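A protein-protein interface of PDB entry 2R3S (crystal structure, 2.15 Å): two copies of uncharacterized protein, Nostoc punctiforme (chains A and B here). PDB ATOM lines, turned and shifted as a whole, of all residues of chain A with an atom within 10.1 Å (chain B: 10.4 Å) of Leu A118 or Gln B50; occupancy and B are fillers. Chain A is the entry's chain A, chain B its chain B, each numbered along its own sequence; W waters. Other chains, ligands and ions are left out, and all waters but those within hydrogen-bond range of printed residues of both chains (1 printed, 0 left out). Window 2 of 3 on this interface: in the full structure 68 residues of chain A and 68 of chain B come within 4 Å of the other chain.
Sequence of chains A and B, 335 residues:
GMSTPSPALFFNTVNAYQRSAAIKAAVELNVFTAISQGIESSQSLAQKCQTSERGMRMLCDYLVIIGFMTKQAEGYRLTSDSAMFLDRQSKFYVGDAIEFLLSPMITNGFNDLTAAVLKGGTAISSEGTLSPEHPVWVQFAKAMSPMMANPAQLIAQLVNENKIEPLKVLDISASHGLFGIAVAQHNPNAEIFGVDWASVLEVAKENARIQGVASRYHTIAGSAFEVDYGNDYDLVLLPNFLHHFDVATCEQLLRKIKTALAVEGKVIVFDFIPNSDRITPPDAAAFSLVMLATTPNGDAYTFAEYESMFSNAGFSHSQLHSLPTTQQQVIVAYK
NH1 of Arg B54 sits at hydrogen-bond distance from O of Gly A120. The side-chain hydroxyl (OG) of Ser B52 sits at hydrogen-bond distance from the backbone carbonyl oxygen (O) of Val A117, 2.7 Å away. The backbone carbonyl oxygen (O) of Leu A118 sits at hydrogen-bond distance from the backbone NH (N) of Ser B52. The side-chain hydroxyl (OG1) of Thr A114 lies within hydrogen-bond range of the side-chain carboxylate (OE1) of Glu B28, at 2.7 Å. N of Gly A120 sits close to OG of Ser B52 (3.3 Å).
The backbone carbonyl oxygen of Leu B29 sits at hydrogen-bond distance from the side-chain sulfur of Cys B49, at 3.5 Å. The backbone NH of Thr A122 sits at hydrogen-bond distance from the backbone carbonyl oxygen of Leu A292 (3.1 Å). The backbone NH (N) of Gly B55 is in hydrogen-bond range of the side-chain hydroxyl (OG) of Ser B52 (3.0 Å). The backbone NH (N) of Thr B51 sits at hydrogen-bond distance from the backbone carbonyl oxygen (O) of Ala B46, 3.0 Å away.
OG1 of Thr A114 touches CA of Ala B25, 3.3 Å away. Leu B29 touches Thr A114 (CD2 to CG2, 3.7 Å). Val A117 touches Leu B29 (CG1 to CD1, 3.5 Å). O of Val A117 touches CB of Thr B51 (3.7 Å). Val A117 touches Gly B55 (CG1 to C, 3.7 Å). Val A117 touches Met B56 (CG1 to N, 3.9 Å). Gln B50 touches Leu A118 (O to CD2, 3.3 Å). Leu A118 touches Thr B51 (O to C, 3.9 Å). N of Leu A292 touches CE of Met B58, at 3.8 Å. Arg B54 touches Pro A296.
Of the printed residues of chain B, Thr A114 touches Ala B25 (3.3 Å), Glu B28 (2.7 Å) and Leu B29 (3.7 Å). No residue of chain B comes within 4 Å of Ala A115. No residue of chain B comes within 4 Å of Ala A116. Of chain B, only Leu B29 (3.5 Å), Thr B51 (3.7 Å), Ser B52 (2.7 Å), Gly B55 (3.7 Å) and Met B56 (3.9 Å) come within 4 Å of Val A117. Of the printed residues of chain B, Leu A118 touches Gln B50 (3.3 Å), Thr B51 (3.9 Å) and Ser B52 (3.2 Å). Thr A122 touches none of the printed residues of chain B. No residue of chain A comes within 4 Å of Cys B49. Of the printed residues of chain A, Gln B50 touches Leu A118 (3.3 Å). Of chain A, only Val A117 (3.7 Å) and Leu A118 (3.9 Å) come within 4 Å of Thr B51. Of chain A, only Val A117 (2.7 Å), Leu A118 (3.2 Å) and Gly A120 (3.1 Å) come within 4 Å of Ser B52. Printed residues of chain A within 4 Å of Met B58: Leu A292. The nearest printed residue of chain B that does not touch Leu A118 is Leu B29 (4.05 Å). The nearest printed residue of chain A that does not touch Gln B50 is Val A117 (6.5 Å). The nearest printed residue of chain A that does not touch Glu B28 is Asp A112 (4.8 Å).
Of the 26 printed residues of chain B, 10 touch a printed residue of chain A. Printed residues of chain B that touch a printed residue of chain A: Ala B25, Glu B28, Leu B29, Gln B50, Thr B51, Ser B52, Arg B54, Gly B55, Met B56 and Met B58. Printed residues of chain A that touch a printed residue of chain B: Thr A114, Val A117, Leu A118, Gly A120, Leu A292 and Pro A296.
No position is printed for both chains. Of the 15 pairs that touch across the chains among the printed residues, none has its exchanged pair printed and touching as well.
Water W1 lies within hydrogen-bond range of OG1 of Thr A114, OD1 of Asp A112 and OE1 of Glu B28.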
ATOM      1  N   ASP A 112      29.170 -18.293  22.224  1.00  0.00           N
ATOM      2  CA  ASP A 112      28.613 -17.151  22.977  1.00  0.00           C
ATOM      3  C   ASP A 112      27.213 -16.827  22.495  1.00  0.00           C
ATOM      4  O   ASP A 112      26.983 -15.894  21.740  1.00  0.00           O
ATOM      5  CB  ASP A 112      29.523 -15.914  22.906  1.00  0.00           C
ATOM      6  CG  ASP A 112      29.372 -14.966  24.146  1.00  0.00           C
ATOM      7  OD1 ASP A 112      28.424 -15.092  24.970  1.00  0.00           O
ATOM      8  OD2 ASP A 112      30.256 -14.095  24.289  1.00  0.00           O
ATOM      9  N   LEU A 113      26.277 -17.638  22.952  1.00  0.00           N
ATOM     10  CA  LEU A 113      24.881 -17.445  22.673  1.00  0.00           C
ATOM     11  C   LEU A 113      24.391 -16.227  23.437  1.00  0.00           C
ATOM     12  O   LEU A 113      23.487 -15.542  22.969  1.00  0.00           O
ATOM     13  CB  LEU A 113      24.113 -18.706  23.043  1.00  0.00           C
ATOM     14  CG  LEU A 113      22.742 -18.978  22.464  1.00  0.00           C
ATOM     15  CD1 LEU A 113      22.729 -18.887  20.940  1.00  0.00           C
ATOM     16  CD2 LEU A 113      22.306 -20.365  22.952  1.00  0.00           C
ATOM     17  N   THR A 114      25.011 -15.916  24.578  1.00  0.00           N
ATOM     18  CA  THR A 114      24.657 -14.704  25.310  1.00  0.00           C
ATOM     19  C   THR A 114      24.814 -13.480  24.429  1.00  0.00           C
ATOM     20  O   THR A 114      23.938 -12.623  24.414  1.00  0.00           O
ATOM     21  CB  THR A 114      25.473 -14.506  26.582  1.00  0.00           C
ATOM     22  OG1 THR A 114      25.357 -15.675  27.415  1.00  0.00           O
ATOM     23  CG2 THR A 114      24.959 -13.280  27.346  1.00  0.00           C
ATOM     24  N   ALA A 115      25.926 -13.423  23.691  1.00  0.00           N
ATOM     25  CA  ALA A 115      26.224 -12.364  22.737  1.00  0.00           C
ATOM     26  C   ALA A 115      25.151 -12.258  21.669  1.00  0.00           C
ATOM     27  O   ALA A 115      24.711 -11.156  21.348  1.00  0.00           O
ATOM     28  CB  ALA A 115      27.593 -12.599  22.079  1.00  0.00           C
ATOM     29  N   ALA A 116      24.755 -13.394  21.097  1.00  0.00           N
ATOM     30  CA  ALA A 116      23.680 -13.419  20.103  1.00  0.00           C
ATOM     31  C   ALA A 116      22.336 -12.956  20.643  1.00  0.00           C
ATOM     32  O   ALA A 116      21.582 -12.271  19.950  1.00  0.00           O
ATOM     33  CB  ALA A 116      23.537 -14.839  19.477  1.00  0.00           C
ATOM     34  N   VAL A 117      21.998 -13.355  21.854  1.00  0.00           N
ATOM     35  CA  VAL A 117      20.729 -12.916  22.465  1.00  0.00           C
ATOM     36  C   VAL A 117      20.770 -11.414  22.705  1.00  0.00           C
ATOM     37  O   VAL A 117      19.809 -10.691  22.428  1.00  0.00           O
ATOM     38  CB  VAL A 117      20.427 -13.671  23.800  1.00  0.00           C
ATOM     39  CG1 VAL A 117      19.200 -13.081  24.471  1.00  0.00           C
ATOM     40  CG2 VAL A 117      20.278 -15.178  23.547  1.00  0.00           C
ATOM     41  N   LEU A 118      21.913 -10.926  23.162  1.00  0.00           N
ATOM     42  CA  LEU A 118      22.081  -9.497  23.415  1.00  0.00           C
ATOM     43  C   LEU A 118      21.868  -8.655  22.165  1.00  0.00           C
ATOM     44  O   LEU A 118      21.163  -7.655  22.206  1.00  0.00           O
ATOM     45  CB  LEU A 118      23.473  -9.209  23.995  1.00  0.00           C
ATOM     46  CG  LEU A 118      23.601  -9.339  25.503  1.00  0.00           C
ATOM     47  CD1 LEU A 118      25.081  -9.176  25.909  1.00  0.00           C
ATOM     48  CD2 LEU A 118      22.719  -8.299  26.251  1.00  0.00           C
ATOM     49  N   LYS A 119      22.456  -9.086  21.052  1.00  0.00           N
ATOM     50  CA  LYS A 119      22.476  -8.285  19.843  1.00  0.00           C
ATOM     51  C   LYS A 119      21.361  -8.597  18.847  1.00  0.00           C
ATOM     52  O   LYS A 119      21.098  -7.784  17.953  1.00  0.00           O
ATOM     53  CB  LYS A 119      23.866  -8.351  19.182  1.00  0.00           C
ATOM     54  CG  LYS A 119      24.228  -9.630  18.432  1.00  0.00           C
ATOM     55  CD  LYS A 119      25.641  -9.505  17.790  1.00  0.00           C
ATOM     56  CE  LYS A 119      25.612  -8.780  16.428  1.00  0.00           C
ATOM     57  NZ  LYS A 119      26.925  -8.763  15.708  1.00  0.00           N
ATOM     58  N   GLY A 120      20.702  -9.747  19.004  1.00  0.00           N
ATOM     59  CA  GLY A 120      19.534 -10.129  18.181  1.00  0.00           C
ATOM     60  C   GLY A 120      19.876 -10.906  16.915  1.00  0.00           C
ATOM     61  O   GLY A 120      19.145 -10.883  15.925  1.00  0.00           O
ATOM     62  N   GLY A 121      21.007 -11.584  16.938  1.00  0.00           N
ATOM     63  CA  GLY A 121      21.473 -12.328  15.793  1.00  0.00           C
ATOM     64  C   GLY A 121      22.895 -12.759  16.025  1.00  0.00           C
ATOM     65  O   GLY A 121      23.471 -12.455  17.069  1.00  0.00           O
ATOM     66  N   THR A 122      23.469 -13.441  15.043  1.00  0.00           N
ATOM     67  CA  THR A 122      24.751 -14.105  15.221  1.00  0.00           C
ATOM     68  C   THR A 122      25.857 -13.139  15.677  1.00  0.00           C
ATOM     69  O   THR A 122      26.004 -12.065  15.135  1.00  0.00           O
ATOM     70  CB  THR A 122      25.224 -14.876  13.948  1.00  0.00           C
ATOM     71  OG1 THR A 122      26.372 -15.664  14.283  1.00  0.00           O
ATOM     72  CG2 THR A 122      25.599 -13.919  12.810  1.00  0.00           C
ATOM     73  N   ALA A 123      26.597 -13.565  16.697  1.00  0.00           N
ATOM     74  CA  ALA A 123      27.817 -12.919  17.153  1.00  0.00           C
ATOM     75  C   ALA A 123      29.063 -13.350  16.335  1.00  0.00           C
ATOM     76  O   ALA A 123      30.174 -12.877  16.600  1.00  0.00           O
ATOM     77  CB  ALA A 123      28.036 -13.255  18.621  1.00  0.00           C
ATOM     78  N   LEU A 292      19.350 -18.086  15.294  1.00  0.00           N
ATOM     79  CA  LEU A 292      19.906 -17.000  16.103  1.00  0.00           C
ATOM     80  C   LEU A 292      21.421 -17.100  16.199  1.00  0.00           C
ATOM     81  O   LEU A 292      22.137 -16.083  16.111  1.00  0.00           O
ATOM     82  CB  LEU A 292      19.294 -16.975  17.510  1.00  0.00           C
ATOM     83  CG  LEU A 292      19.836 -15.965  18.533  1.00  0.00           C
ATOM     84  CD1 LEU A 292      19.488 -14.504  18.199  1.00  0.00           C
ATOM     85  CD2 LEU A 292      19.349 -16.315  19.919  1.00  0.00           C
ATOM     86  N   ALA A 293      21.912 -18.314  16.442  1.00  0.00           N
ATOM     87  CA  ALA A 293      23.336 -18.504  16.670  1.00  0.00           C
ATOM     88  C   ALA A 293      24.182 -18.270  15.415  1.00  0.00           C
ATOM     89  O   ALA A 293      25.317 -17.832  15.521  1.00  0.00           O
ATOM     90  CB  ALA A 293      23.637 -19.895  17.265  1.00  0.00           C
ATOM     91  N   PRO A 296      22.360 -13.571  10.851  1.00  0.00           N
ATOM     92  CA  PRO A 296      21.984 -12.272  11.443  1.00  0.00           C
ATOM     93  C   PRO A 296      20.492 -12.050  11.729  1.00  0.00           C
ATOM     94  O   PRO A 296      20.192 -11.410  12.710  1.00  0.00           O
ATOM     95  CB  PRO A 296      22.518 -11.232  10.415  1.00  0.00           C
ATOM     96  CG  PRO A 296      23.541 -12.014   9.576  1.00  0.00           C
ATOM     97  CD  PRO A 296      22.937 -13.405   9.502  1.00  0.00           C
ATOM     98  N   ALA B  25      23.338 -19.049  28.576  1.00  0.00           N
ATOM     99  CA  ALA B  25      22.886 -17.693  28.242  1.00  0.00           C
ATOM    100  C   ALA B  25      21.806 -17.203  29.226  1.00  0.00           C
ATOM    101  O   ALA B  25      21.851 -16.045  29.708  1.00  0.00           O
ATOM    102  CB  ALA B  25      22.407 -17.626  26.791  1.00  0.00           C
ATOM    103  N   ALA B  26      20.851 -18.079  29.529  1.00  0.00           N
ATOM    104  CA  ALA B  26      19.726 -17.766  30.420  1.00  0.00           C
ATOM    105  C   ALA B  26      20.155 -17.416  31.854  1.00  0.00           C
ATOM    106  O   ALA B  26      19.603 -16.490  32.481  1.00  0.00           O
ATOM    107  CB  ALA B  26      18.712 -18.923  30.426  1.00  0.00           C
ATOM    108  N   GLU B  28      23.357 -16.437  32.702  1.00  0.00           N
ATOM    109  CA  GLU B  28      24.150 -15.210  32.587  1.00  0.00           C
ATOM    110  C   GLU B  28      23.314 -13.973  32.415  1.00  0.00           C
ATOM    111  O   GLU B  28      23.708 -12.907  32.895  1.00  0.00           O
ATOM    112  CB  GLU B  28      25.173 -15.312  31.435  1.00  0.00           C
ATOM    113  CG  GLU B  28      26.352 -16.254  31.771  1.00  0.00           C
ATOM    114  CD  GLU B  28      27.399 -16.355  30.663  1.00  0.00           C
ATOM    115  OE1 GLU B  28      27.111 -15.978  29.503  1.00  0.00           O
ATOM    116  OE2 GLU B  28      28.513 -16.820  30.976  1.00  0.00           O
ATOM    117  N   LEU B  29      22.179 -14.104  31.735  1.00  0.00           N
ATOM    118  CA  LEU B  29      21.298 -12.967  31.458  1.00  0.00           C
ATOM    119  C   LEU B  29      20.246 -12.785  32.529  1.00  0.00           C
ATOM    120  O   LEU B  29      19.513 -11.790  32.536  1.00  0.00           O
ATOM    121  CB  LEU B  29      20.630 -13.074  30.069  1.00  0.00           C
ATOM    122  CG  LEU B  29      21.545 -12.891  28.852  1.00  0.00           C
ATOM    123  CD1 LEU B  29      20.843 -13.305  27.581  1.00  0.00           C
ATOM    124  CD2 LEU B  29      22.070 -11.447  28.713  1.00  0.00           C
ATOM    125  N   ASN B  30      20.189 -13.728  33.451  1.00  0.00           N
ATOM    126  CA  ASN B  30      19.311 -13.627  34.606  1.00  0.00           C
ATOM    127  C   ASN B  30      17.852 -13.716  34.264  1.00  0.00           C
ATOM    128  O   ASN B  30      17.016 -13.096  34.928  1.00  0.00           O
ATOM    129  CB  ASN B  30      19.571 -12.329  35.344  1.00  0.00           C
ATOM    130  CG  ASN B  30      20.319 -12.546  36.571  1.00  0.00           C
ATOM    131  OD1 ASN B  30      19.754 -12.429  37.667  1.00  0.00           O
ATOM    132  ND2 ASN B  30      21.609 -12.893  36.430  1.00  0.00           N
ATOM    133  N   VAL B  31      17.555 -14.542  33.264  1.00  0.00           N
ATOM    134  CA  VAL B  31      16.217 -14.662  32.749  1.00  0.00           C
ATOM    135  C   VAL B  31      15.247 -15.194  33.809  1.00  0.00           C
ATOM    136  O   VAL B  31      14.156 -14.679  33.952  1.00  0.00           O
ATOM    137  CB  VAL B  31      16.192 -15.549  31.455  1.00  0.00           C
ATOM    138  CG1 VAL B  31      14.756 -15.760  31.011  1.00  0.00           C
ATOM    139  CG2 VAL B  31      17.029 -14.883  30.331  1.00  0.00           C
ATOM    140  N   ALA B  34      14.236 -12.738  36.334  1.00  0.00           N
ATOM    141  CA  ALA B  34      13.320 -11.751  35.765  1.00  0.00           C
ATOM    142  C   ALA B  34      11.887 -12.244  35.644  1.00  0.00           C
ATOM    143  O   ALA B  34      10.950 -11.459  35.797  1.00  0.00           O
ATOM    144  CB  ALA B  34      13.817 -11.255  34.419  1.00  0.00           C
ATOM    145  N   SER B  41       6.276 -11.372  29.181  1.00  0.00           N
ATOM    146  CA  SER B  41       6.435 -11.474  27.744  1.00  0.00           C
ATOM    147  C   SER B  41       7.908 -11.424  27.369  1.00  0.00           C
ATOM    148  O   SER B  41       8.757 -11.034  28.182  1.00  0.00           O
ATOM    149  CB  SER B  41       5.709 -10.304  27.073  1.00  0.00           C
ATOM    150  OG  SER B  41       6.340  -9.082  27.390  1.00  0.00           O
ATOM    151  N   SER B  42       8.223 -11.801  26.137  1.00  0.00           N
ATOM    152  CA  SER B  42       9.605 -11.660  25.676  1.00  0.00           C
ATOM    153  C   SER B  42       9.999 -10.184  25.575  1.00  0.00           C
ATOM    154  O   SER B  42      11.141  -9.854  25.765  1.00  0.00           O
ATOM    155  CB  SER B  42       9.861 -12.411  24.367  1.00  0.00           C
ATOM    156  OG  SER B  42       8.958 -12.034  23.369  1.00  0.00           O
ATOM    157  N   GLN B  43       9.038  -9.299  25.343  1.00  0.00           N
ATOM    158  CA  GLN B  43       9.329  -7.855  25.274  1.00  0.00           C
ATOM    159  C   GLN B  43       9.681  -7.324  26.655  1.00  0.00           C
ATOM    160  O   GLN B  43      10.645  -6.594  26.818  1.00  0.00           O
ATOM    161  CB  GLN B  43       8.137  -7.062  24.735  1.00  0.00           C
ATOM    162  CG  GLN B  43       8.435  -5.577  24.488  1.00  0.00           C
ATOM    163  CD  GLN B  43       9.460  -5.380  23.389  1.00  0.00           C
ATOM    164  OE1 GLN B  43      10.522  -4.776  23.600  1.00  0.00           O
ATOM    165  NE2 GLN B  43       9.159  -5.917  22.206  1.00  0.00           N
ATOM    166  N   SER B  44       8.890  -7.693  27.655  1.00  0.00           N
ATOM    167  CA  SER B  44       9.182  -7.329  29.032  1.00  0.00           C
ATOM    168  C   SER B  44      10.550  -7.852  29.483  1.00  0.00           C
ATOM    169  O   SER B  44      11.326  -7.139  30.099  1.00  0.00           O
ATOM    170  CB  SER B  44       8.098  -7.898  29.936  1.00  0.00           C
ATOM    171  OG  SER B  44       8.404  -7.664  31.282  1.00  0.00           O
ATOM    172  N   LEU B  45      10.818  -9.114  29.198  1.00  0.00           N
ATOM    173  CA  LEU B  45      12.085  -9.728  29.563  1.00  0.00           C
ATOM    174  C   LEU B  45      13.286  -9.086  28.861  1.00  0.00           C
ATOM    175  O   LEU B  45      14.337  -8.955  29.474  1.00  0.00           O
ATOM    176  CB  LEU B  45      12.034 -11.223  29.280  1.00  0.00           C
ATOM    177  CG  LEU B  45      11.131 -12.036  30.215  1.00  0.00           C
ATOM    178  CD1 LEU B  45      11.052 -13.458  29.734  1.00  0.00           C
ATOM    179  CD2 LEU B  45      11.587 -11.981  31.686  1.00  0.00           C
ATOM    180  N   ALA B  46      13.123  -8.658  27.600  1.00  0.00           N
ATOM    181  CA  ALA B  46      14.174  -7.952  26.860  1.00  0.00           C
ATOM    182  C   ALA B  46      14.507  -6.637  27.547  1.00  0.00           C
ATOM    183  O   ALA B  46      15.683  -6.267  27.680  1.00  0.00           O
ATOM    184  CB  ALA B  46      13.742  -7.687  25.418  1.00  0.00           C
ATOM    185  N   GLN B  47      13.470  -5.929  27.980  1.00  0.00           N
ATOM    186  CA  GLN B  47      13.656  -4.703  28.734  1.00  0.00           C
ATOM    187  C   GLN B  47      14.311  -4.960  30.107  1.00  0.00           C
ATOM    188  O   GLN B  47      15.219  -4.234  30.503  1.00  0.00           O
ATOM    189  CB  GLN B  47      12.310  -3.950  28.872  1.00  0.00           C
ATOM    190  CG  GLN B  47      11.787  -3.282  27.572  1.00  0.00           C
ATOM    191  N   LYS B  48      13.850  -5.973  30.842  1.00  0.00           N
ATOM    192  CA  LYS B  48      14.422  -6.255  32.167  1.00  0.00           C
ATOM    193  C   LYS B  48      15.879  -6.723  32.097  1.00  0.00           C
ATOM    194  O   LYS B  48      16.686  -6.359  32.934  1.00  0.00           O
ATOM    195  CB  LYS B  48      13.594  -7.298  32.906  1.00  0.00           C
ATOM    196  CG  LYS B  48      12.305  -6.745  33.455  1.00  0.00           C
ATOM    197  CD  LYS B  48      11.310  -7.835  33.754  1.00  0.00           C
ATOM    198  CE  LYS B  48      10.264  -7.372  34.772  1.00  0.00           C
ATOM    199  NZ  LYS B  48      10.428  -8.168  36.054  1.00  0.00           N
ATOM    200  N   CYS B  49      16.196  -7.510  31.079  1.00  0.00           N
ATOM    201  CA  CYS B  49      17.508  -8.132  30.930  1.00  0.00           C
ATOM    202  C   CYS B  49      18.459  -7.390  29.978  1.00  0.00           C
ATOM    203  O   CYS B  49      19.607  -7.809  29.813  1.00  0.00           O
ATOM    204  CB  CYS B  49      17.313  -9.578  30.451  1.00  0.00           C
ATOM    205  SG  CYS B  49      16.325 -10.597  31.606  1.00  0.00           S
ATOM    206  N   GLN B  50      17.932  -6.345  29.336  1.00  0.00           N
ATOM    207  CA  GLN B  50      18.703  -5.461  28.475  1.00  0.00           C
ATOM    208  C   GLN B  50      19.264  -6.184  27.221  1.00  0.00           C
ATOM    209  O   GLN B  50      20.441  -6.014  26.867  1.00  0.00           O
ATOM    210  CB  GLN B  50      19.792  -4.742  29.317  1.00  0.00           C
ATOM    211  CG  GLN B  50      19.223  -4.014  30.580  1.00  0.00           C
ATOM    212  CD  GLN B  50      20.280  -3.623  31.647  1.00  0.00           C
ATOM    213  OE1 GLN B  50      20.383  -2.450  32.044  1.00  0.00           O
ATOM    214  NE2 GLN B  50      21.039  -4.605  32.124  1.00  0.00           N
ATOM    215  N   THR B  51      18.410  -6.969  26.560  1.00  0.00           N
ATOM    216  CA  THR B  51      18.762  -7.745  25.364  1.00  0.00           C
ATOM    217  C   THR B  51      17.841  -7.336  24.229  1.00  0.00           C
ATOM    218  O   THR B  51      16.894  -6.594  24.443  1.00  0.00           O
ATOM    219  CB  THR B  51      18.532  -9.254  25.592  1.00  0.00           C
ATOM    220  OG1 THR B  51      17.144  -9.541  25.458  1.00  0.00           O
ATOM    221  CG2 THR B  51      18.980  -9.670  26.959  1.00  0.00           C
ATOM    222  N   SER B  52      18.109  -7.831  23.024  1.00  0.00           N
ATOM    223  CA  SER B  52      17.146  -7.755  21.911  1.00  0.00           C
ATOM    224  C   SER B  52      15.831  -8.486  22.230  1.00  0.00           C
ATOM    225  O   SER B  52      15.818  -9.488  22.956  1.00  0.00           O
ATOM    226  CB  SER B  52      17.740  -8.385  20.641  1.00  0.00           C
ATOM    227  OG  SER B  52      17.893  -9.801  20.804  1.00  0.00           O
ATOM    228  N   GLU B  53      14.723  -8.011  21.663  1.00  0.00           N
ATOM    229  CA  GLU B  53      13.464  -8.739  21.803  1.00  0.00           C
ATOM    230  C   GLU B  53      13.522 -10.110  21.099  1.00  0.00           C
ATOM    231  O   GLU B  53      13.092 -11.111  21.675  1.00  0.00           O
ATOM    232  CB  GLU B  53      12.271  -7.914  21.305  1.00  0.00           C
ATOM    233  CG  GLU B  53      10.870  -8.563  21.589  1.00  0.00           C
ATOM    234  CD  GLU B  53      10.510  -9.791  20.698  1.00  0.00           C
ATOM    235  OE1 GLU B  53      11.008  -9.885  19.548  1.00  0.00           O
ATOM    236  OE2 GLU B  53       9.715 -10.666  21.153  1.00  0.00           O
ATOM    237  N   ARG B  54      14.036 -10.182  19.868  1.00  0.00           N
ATOM    238  CA  ARG B  54      13.982 -11.456  19.138  1.00  0.00           C
ATOM    239  C   ARG B  54      14.906 -12.494  19.768  1.00  0.00           C
ATOM    240  O   ARG B  54      14.560 -13.650  19.835  1.00  0.00           O
ATOM    241  CB  ARG B  54      14.257 -11.293  17.637  1.00  0.00           C
ATOM    242  CG  ARG B  54      15.673 -10.945  17.277  1.00  0.00           C
ATOM    243  CD  ARG B  54      15.776 -10.485  15.818  1.00  0.00           C
ATOM    244  NE  ARG B  54      15.303 -11.534  14.910  1.00  0.00           N
ATOM    245  CZ  ARG B  54      16.025 -12.568  14.487  1.00  0.00           C
ATOM    246  NH1 ARG B  54      17.307 -12.725  14.826  1.00  0.00           N
ATOM    247  NH2 ARG B  54      15.465 -13.437  13.666  1.00  0.00           N
ATOM    248  N   GLY B  55      16.055 -12.063  20.269  1.00  0.00           N
ATOM    249  CA  GLY B  55      16.961 -12.957  20.972  1.00  0.00           C
ATOM    250  C   GLY B  55      16.301 -13.587  22.186  1.00  0.00           C
ATOM    251  O   GLY B  55      16.400 -14.792  22.401  1.00  0.00           O
ATOM    252  N   MET B  56      15.626 -12.757  22.977  1.00  0.00           N
ATOM    253  CA  MET B  56      14.910 -13.220  24.175  1.00  0.00           C
ATOM    254  C   MET B  56      13.789 -14.189  23.830  1.00  0.00           C
ATOM    255  O   MET B  56      13.618 -15.206  24.502  1.00  0.00           O
ATOM    256  CB  MET B  56      14.338 -12.022  24.941  1.00  0.00           C
ATOM    257  CG  MET B  56      13.711 -12.349  26.304  1.00  0.00           C
ATOM    258  SD  MET B  56      14.970 -13.281  27.529  1.00  0.00           S
ATOM    259  CE  MET B  56      16.221 -11.814  27.958  1.00  0.00           C
ATOM    260  N   ARG B  57      13.008 -13.855  22.798  1.00  0.00           N
ATOM    261  CA  ARG B  57      11.913 -14.705  22.365  1.00  0.00           C
ATOM    262  C   ARG B  57      12.436 -16.072  21.925  1.00  0.00           C
ATOM    263  O   ARG B  57      11.890 -17.093  22.285  1.00  0.00           O
ATOM    264  CB  ARG B  57      11.158 -14.019  21.222  1.00  0.00           C
ATOM    265  CG  ARG B  57      10.022 -14.844  20.607  1.00  0.00           C
ATOM    266  CD  ARG B  57      10.475 -15.731  19.442  1.00  0.00           C
ATOM    267  NE  ARG B  57      10.745 -14.911  18.268  1.00  0.00           N
ATOM    268  CZ  ARG B  57      11.135 -15.374  17.086  1.00  0.00           C
ATOM    269  NH1 ARG B  57      11.311 -16.675  16.894  1.00  0.00           N
ATOM    270  NH2 ARG B  57      11.356 -14.515  16.095  1.00  0.00           N
ATOM    271  N   MET B  58      13.495 -16.075  21.121  1.00  0.00           N
ATOM    272  CA  MET B  58      14.024 -17.309  20.579  1.00  0.00           C
ATOM    273  C   MET B  58      14.607 -18.197  21.660  1.00  0.00           C
ATOM    274  O   MET B  58      14.395 -19.420  21.624  1.00  0.00           O
ATOM    275  CB  MET B  58      15.041 -17.016  19.471  1.00  0.00           C
ATOM    276  CG  MET B  58      14.386 -16.294  18.298  1.00  0.00           C
ATOM    277  SD  MET B  58      15.598 -15.240  17.151  1.00  0.00           S
ATOM    278  CE  MET B  58      15.942 -16.539  15.760  1.00  0.00           C
ATOM    279  N   LEU B  59      15.314 -17.584  22.614  1.00  0.00           N
ATOM    280  CA  LEU B  59      15.856 -18.276  23.793  1.00  0.00           C
ATOM    281  C   LEU B  59      14.745 -18.806  24.706  1.00  0.00           C
ATOM    282  O   LEU B  59      14.764 -19.970  25.121  1.00  0.00           O
ATOM    283  CB  LEU B  59      16.812 -17.348  24.592  1.00  0.00           C
ATOM    284  CG  LEU B  59      17.496 -17.895  25.868  1.00  0.00           C
ATOM    285  CD1 LEU B  59      18.470 -19.014  25.523  1.00  0.00           C
ATOM    286  CD2 LEU B  59      18.206 -16.803  26.688  1.00  0.00           C
HETATM  287  O   HOH W   1      27.045 -17.352  26.595  1.00  0.00           O
